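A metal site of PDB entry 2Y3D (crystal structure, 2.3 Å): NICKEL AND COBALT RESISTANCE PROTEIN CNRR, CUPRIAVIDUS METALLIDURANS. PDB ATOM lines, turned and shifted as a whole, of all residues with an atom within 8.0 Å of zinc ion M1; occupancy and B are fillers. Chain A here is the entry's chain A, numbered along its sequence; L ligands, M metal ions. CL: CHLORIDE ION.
The side-chain carboxylate (OE1) of Glu 33 sits close to a ring nitrogen (ND1) of His 12, at 3.2 Å.
His 12 touches zinc ion M1 (ND1 to ZN, 3.9 Å).
Four residues have an atom within 4 Å of zinc ion M1: His 8, His 12, Glu 33 and His 89.
Zinc ion M1 is bound by a ring nitrogen (NE2) of His 89, the side-chain carboxylate (OE1) of Glu 33, a ring nitrogen (NE2) of His 8 and a chlorine (CL) of the ligand.
Zinc ion M1 has four donor atoms within binding distance.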
ATOM      1  N   HIS A   8      30.932  13.373   6.723  1.00  0.00           N
ATOM      2  CA  HIS A   8      29.498  13.587   6.892  1.00  0.00           C
ATOM      3  C   HIS A   8      28.952  14.597   5.893  1.00  0.00           C
ATOM      4  O   HIS A   8      28.056  14.266   5.122  1.00  0.00           O
ATOM      5  CB  HIS A   8      29.130  14.025   8.308  1.00  0.00           C
ATOM      6  CG  HIS A   8      27.676  14.351   8.469  1.00  0.00           C
ATOM      7  ND1 HIS A   8      27.215  15.646   8.566  1.00  0.00           N
ATOM      8  CD2 HIS A   8      26.580  13.549   8.501  1.00  0.00           C
ATOM      9  CE1 HIS A   8      25.893  15.624   8.677  1.00  0.00           C
ATOM     10  NE2 HIS A   8      25.491  14.365   8.634  1.00  0.00           N
ATOM     11  N   GLY A   9      29.501  15.806   5.920  1.00  0.00           N
ATOM     12  CA  GLY A   9      29.093  16.858   5.001  1.00  0.00           C
ATOM     13  C   GLY A   9      28.893  16.360   3.583  1.00  0.00           C
ATOM     14  O   GLY A   9      27.837  16.570   2.986  1.00  0.00           O
ATOM     15  N   LEU A  11      28.669  13.204   2.508  1.00  0.00           N
ATOM     16  CA  LEU A  11      27.743  12.081   2.406  1.00  0.00           C
ATOM     17  C   LEU A  11      26.298  12.568   2.270  1.00  0.00           C
ATOM     18  O   LEU A  11      25.469  11.954   1.602  1.00  0.00           O
ATOM     19  CB  LEU A  11      27.855  11.176   3.624  1.00  0.00           C
ATOM     20  CG  LEU A  11      29.089  10.280   3.694  1.00  0.00           C
ATOM     21  CD1 LEU A  11      29.275   9.837   5.134  1.00  0.00           C
ATOM     22  CD2 LEU A  11      28.937   9.094   2.762  1.00  0.00           C
ATOM     23  N   HIS A  12      26.009  13.684   2.927  1.00  0.00           N
ATOM     24  CA  HIS A  12      24.670  14.215   2.912  1.00  0.00           C
ATOM     25  C   HIS A  12      24.376  14.776   1.525  1.00  0.00           C
ATOM     26  O   HIS A  12      23.268  14.634   1.014  1.00  0.00           O
ATOM     27  CB  HIS A  12      24.504  15.298   3.985  1.00  0.00           C
ATOM     28  CG  HIS A  12      23.075  15.658   4.263  1.00  0.00           C
ATOM     29  ND1 HIS A  12      22.229  14.830   4.958  1.00  0.00           N
ATOM     30  CD2 HIS A  12      22.354  16.745   3.904  1.00  0.00           C
ATOM     31  CE1 HIS A  12      21.036  15.401   5.027  1.00  0.00           C
ATOM     32  NE2 HIS A  12      21.085  16.557   4.407  1.00  0.00           N
ATOM     33  N   GLU A  13      25.373  15.394   0.904  1.00  0.00           N
ATOM     34  CA  GLU A  13      25.203  15.877  -0.465  1.00  0.00           C
ATOM     35  C   GLU A  13      24.886  14.701  -1.381  1.00  0.00           C
ATOM     36  O   GLU A  13      23.979  14.776  -2.207  1.00  0.00           O
ATOM     37  CB  GLU A  13      26.436  16.638  -0.916  1.00  0.00           C
ATOM     38  CG  GLU A  13      26.504  18.020  -0.284  1.00  0.00           C
ATOM     39  CD  GLU A  13      25.179  18.751  -0.389  1.00  0.00           C
ATOM     40  OE1 GLU A  13      24.647  18.836  -1.523  1.00  0.00           O
ATOM     41  OE2 GLU A  13      24.670  19.232   0.650  1.00  0.00           O
ATOM     42  N   LEU A  15      23.333  12.365  -0.554  1.00  0.00           N
ATOM     43  CA  LEU A  15      21.915  12.148  -0.259  1.00  0.00           C
ATOM     44  C   LEU A  15      21.030  13.151  -0.996  1.00  0.00           C
ATOM     45  O   LEU A  15      20.029  12.772  -1.600  1.00  0.00           O
ATOM     46  CB  LEU A  15      21.655  12.185   1.248  1.00  0.00           C
ATOM     47  CG  LEU A  15      21.586  10.866   2.026  1.00  0.00           C
ATOM     48  CD1 LEU A  15      22.027   9.662   1.195  1.00  0.00           C
ATOM     49  CD2 LEU A  15      22.383  10.946   3.325  1.00  0.00           C
ATOM     50  N   LEU A  29      14.527  11.506   5.381  1.00  0.00           N
ATOM     51  CA  LEU A  29      15.932  11.831   5.440  1.00  0.00           C
ATOM     52  C   LEU A  29      16.188  13.086   6.281  1.00  0.00           C
ATOM     53  O   LEU A  29      17.003  13.065   7.218  1.00  0.00           O
ATOM     54  CB  LEU A  29      16.464  11.966   4.019  1.00  0.00           C
ATOM     55  CG  LEU A  29      17.870  12.400   3.691  1.00  0.00           C
ATOM     56  CD1 LEU A  29      18.189  11.900   2.281  1.00  0.00           C
ATOM     57  CD2 LEU A  29      17.977  13.903   3.753  1.00  0.00           C
ATOM     58  N   GLU A  30      15.465  14.173   5.993  1.00  0.00           N
ATOM     59  CA  GLU A  30      15.712  15.412   6.713  1.00  0.00           C
ATOM     60  C   GLU A  30      15.308  15.384   8.188  1.00  0.00           C
ATOM     61  O   GLU A  30      15.866  16.137   8.993  1.00  0.00           O
ATOM     62  CB  GLU A  30      15.073  16.617   6.012  1.00  0.00           C
ATOM     63  CG  GLU A  30      15.625  16.903   4.627  1.00  0.00           C
ATOM     64  CD  GLU A  30      17.112  17.209   4.609  1.00  0.00           C
ATOM     65  OE1 GLU A  30      17.730  17.427   5.684  1.00  0.00           O
ATOM     66  OE2 GLU A  30      17.650  17.232   3.492  1.00  0.00           O
ATOM     67  N   LYS A  32      15.715  12.650  10.069  1.00  0.00           N
ATOM     68  CA  LYS A  32      16.838  11.945  10.669  1.00  0.00           C
ATOM     69  C   LYS A  32      17.974  12.939  10.849  1.00  0.00           C
ATOM     70  O   LYS A  32      18.649  12.935  11.868  1.00  0.00           O
ATOM     71  CB  LYS A  32      17.267  10.776   9.786  1.00  0.00           C
ATOM     72  CG  LYS A  32      16.327   9.603   9.893  1.00  0.00           C
ATOM     73  CD  LYS A  32      16.623   8.538   8.862  1.00  0.00           C
ATOM     74  CE  LYS A  32      15.646   7.384   9.003  1.00  0.00           C
ATOM     75  NZ  LYS A  32      15.708   6.437   7.871  1.00  0.00           N
ATOM     76  N   GLU A  33      18.136  13.825   9.867  1.00  0.00           N
ATOM     77  CA  GLU A  33      19.184  14.813   9.927  1.00  0.00           C
ATOM     78  C   GLU A  33      18.943  15.788  11.065  1.00  0.00           C
ATOM     79  O   GLU A  33      19.884  16.132  11.775  1.00  0.00           O
ATOM     80  CB  GLU A  33      19.316  15.566   8.600  1.00  0.00           C
ATOM     81  CG  GLU A  33      20.529  16.493   8.560  1.00  0.00           C
ATOM     82  CD  GLU A  33      21.856  15.745   8.565  1.00  0.00           C
ATOM     83  OE1 GLU A  33      21.888  14.590   8.110  1.00  0.00           O
ATOM     84  OE2 GLU A  33      22.876  16.308   8.998  1.00  0.00           O
ATOM     85  N   ASP A  34      17.699  16.242  11.238  1.00  0.00           N
ATOM     86  CA  ASP A  34      17.360  17.140  12.337  1.00  0.00           C
ATOM     87  C   ASP A  34      17.803  16.517  13.656  1.00  0.00           C
ATOM     88  O   ASP A  34      18.373  17.206  14.503  1.00  0.00           O
ATOM     89  CB  ASP A  34      15.853  17.408  12.446  1.00  0.00           C
ATOM     90  CG  ASP A  34      15.280  18.136  11.243  1.00  0.00           C
ATOM     91  OD1 ASP A  34      16.046  18.783  10.507  1.00  0.00           O
ATOM     92  OD2 ASP A  34      14.052  18.074  11.064  1.00  0.00           O
ATOM     93  N   PHE A  36      20.090  14.111  14.262  1.00  0.00           N
ATOM     94  CA  PHE A  36      21.538  14.086  14.355  1.00  0.00           C
ATOM     95  C   PHE A  36      22.128  15.474  14.612  1.00  0.00           C
ATOM     96  O   PHE A  36      23.016  15.603  15.459  1.00  0.00           O
ATOM     97  CB  PHE A  36      22.187  13.477  13.130  1.00  0.00           C
ATOM     98  CG  PHE A  36      23.687  13.629  13.141  1.00  0.00           C
ATOM     99  CD1 PHE A  36      24.457  12.916  14.053  1.00  0.00           C
ATOM    100  CD2 PHE A  36      24.309  14.483  12.248  1.00  0.00           C
ATOM    101  CE1 PHE A  36      25.835  13.061  14.079  1.00  0.00           C
ATOM    102  CE2 PHE A  36      25.684  14.627  12.257  1.00  0.00           C
ATOM    103  CZ  PHE A  36      26.463  13.913  13.173  1.00  0.00           C
ATOM    104  N   ALA A  37      21.660  16.492  13.886  1.00  0.00           N
ATOM    105  CA  ALA A  37      22.138  17.859  14.110  1.00  0.00           C
ATOM    106  C   ALA A  37      22.013  18.268  15.575  1.00  0.00           C
ATOM    107  O   ALA A  37      22.936  18.858  16.140  1.00  0.00           O
ATOM    108  CB  ALA A  37      21.395  18.857  13.203  1.00  0.00           C
ATOM    109  N   ARG A  40      24.528  16.305  17.790  1.00  0.00           N
ATOM    110  CA  ARG A  40      25.865  16.813  17.534  1.00  0.00           C
ATOM    111  C   ARG A  40      26.107  18.115  18.287  1.00  0.00           C
ATOM    112  O   ARG A  40      27.169  18.312  18.885  1.00  0.00           O
ATOM    113  CB  ARG A  40      26.105  17.031  16.046  1.00  0.00           C
ATOM    114  CG  ARG A  40      27.504  17.557  15.744  1.00  0.00           C
ATOM    115  CD  ARG A  40      27.757  17.655  14.255  1.00  0.00           C
ATOM    116  NE  ARG A  40      26.728  18.491  13.650  1.00  0.00           N
ATOM    117  CZ  ARG A  40      26.520  18.609  12.337  1.00  0.00           C
ATOM    118  NH1 ARG A  40      27.276  17.943  11.483  1.00  0.00           N
ATOM    119  NH2 ARG A  40      25.540  19.392  11.908  1.00  0.00           N
ATOM    120  N   THR A  86      28.335  10.239  15.210  1.00  0.00           N
ATOM    121  CA  THR A  86      28.402  10.545  13.782  1.00  0.00           C
ATOM    122  C   THR A  86      28.388   9.282  12.907  1.00  0.00           C
ATOM    123  O   THR A  86      27.673   9.218  11.922  1.00  0.00           O
ATOM    124  CB  THR A  86      29.658  11.357  13.460  1.00  0.00           C
ATOM    125  OG1 THR A  86      29.643  12.565  14.213  1.00  0.00           O
ATOM    126  CG2 THR A  86      29.727  11.694  11.971  1.00  0.00           C
ATOM    127  N   HIS A  89      25.062   7.409  12.916  1.00  0.00           N
ATOM    128  CA  HIS A  89      24.170   8.192  12.069  1.00  0.00           C
ATOM    129  C   HIS A  89      24.430   7.925  10.591  1.00  0.00           C
ATOM    130  O   HIS A  89      23.496   7.647   9.824  1.00  0.00           O
ATOM    131  CB  HIS A  89      24.326   9.676  12.363  1.00  0.00           C
ATOM    132  CG  HIS A  89      23.710  10.575  11.329  1.00  0.00           C
ATOM    133  ND1 HIS A  89      22.368  10.559  11.055  1.00  0.00           N
ATOM    134  CD2 HIS A  89      24.266  11.503  10.525  1.00  0.00           C
ATOM    135  CE1 HIS A  89      22.108  11.459  10.125  1.00  0.00           C
ATOM    136  NE2 HIS A  89      23.235  12.036   9.772  1.00  0.00           N
ATOM    137  N   VAL A  90      25.684   7.994  10.185  1.00  0.00           N
ATOM    138  CA  VAL A  90      26.074   7.686   8.817  1.00  0.00           C
ATOM    139  C   VAL A  90      25.595   6.296   8.343  1.00  0.00           C
ATOM    140  O   VAL A  90      25.151   6.156   7.200  1.00  0.00           O
ATOM    141  CB  VAL A  90      27.594   7.873   8.624  1.00  0.00           C
ATOM    142  CG1 VAL A  90      28.091   7.103   7.415  1.00  0.00           C
ATOM    143  CG2 VAL A  90      27.911   9.341   8.506  1.00  0.00           C
ATOM    144  N   GLU A  92      22.985   4.701   9.613  1.00  0.00           N
ATOM    145  CA  GLU A  92      21.545   4.746   9.599  1.00  0.00           C
ATOM    146  C   GLU A  92      21.076   5.330   8.275  1.00  0.00           C
ATOM    147  O   GLU A  92      20.091   4.863   7.696  1.00  0.00           O
ATOM    148  CB  GLU A  92      21.031   5.608  10.742  1.00  0.00           C
ATOM    149  CG  GLU A  92      19.545   5.767  10.747  1.00  0.00           C
ATOM    150  CD  GLU A  92      19.074   6.830  11.719  1.00  0.00           C
ATOM    151  OE1 GLU A  92      19.760   7.893  11.848  1.00  0.00           O
ATOM    152  OE2 GLU A  92      18.021   6.613  12.369  1.00  0.00           O
ATOM    153  N   MET A  93      21.774   6.366   7.811  1.00  0.00           N
ATOM    154  CA  MET A  93      21.397   7.055   6.589  1.00  0.00           C
ATOM    155  C   MET A  93      21.610   6.141   5.394  1.00  0.00           C
ATOM    156  O   MET A  93      20.840   6.180   4.442  1.00  0.00           O
ATOM    157  CB  MET A  93      22.162   8.363   6.405  1.00  0.00           C
ATOM    158  CG  MET A  93      21.919   9.405   7.481  1.00  0.00           C
ATOM    159  SD  MET A  93      20.187   9.675   7.920  1.00  0.00           S
ATOM    160  CE  MET A  93      19.705  10.793   6.588  1.00  0.00           C
ATOM    161  N   TYR A 105      28.167   6.166  -2.073  1.00  0.00           N
ATOM    162  CA  TYR A 105      28.118   6.560  -0.673  1.00  0.00           C
ATOM    163  C   TYR A 105      29.256   5.889   0.110  1.00  0.00           C
ATOM    164  O   TYR A 105      30.007   6.555   0.841  1.00  0.00           O
ATOM    165  CB  TYR A 105      26.759   6.157  -0.114  1.00  0.00           C
ATOM    166  CG  TYR A 105      26.433   6.663   1.268  1.00  0.00           C
ATOM    167  CD1 TYR A 105      25.924   7.947   1.455  1.00  0.00           C
ATOM    168  CD2 TYR A 105      26.581   5.849   2.382  1.00  0.00           C
ATOM    169  CE1 TYR A 105      25.604   8.413   2.721  1.00  0.00           C
ATOM    170  CE2 TYR A 105      26.258   6.293   3.643  1.00  0.00           C
ATOM    171  CZ  TYR A 105      25.766   7.565   3.817  1.00  0.00           C
ATOM    172  OH  TYR A 105      25.444   7.995   5.097  1.00  0.00           O
HETATM  173 CL    CL L   1      23.658  12.376   6.249  1.00  0.00          CL
HETATM  174 ZN    ZN M   1      23.631  13.434   8.290  1.00  0.00          ZN
HETATM  175 ZN    ZN M   2      19.631  17.929   3.582  1.00  0.00          ZN
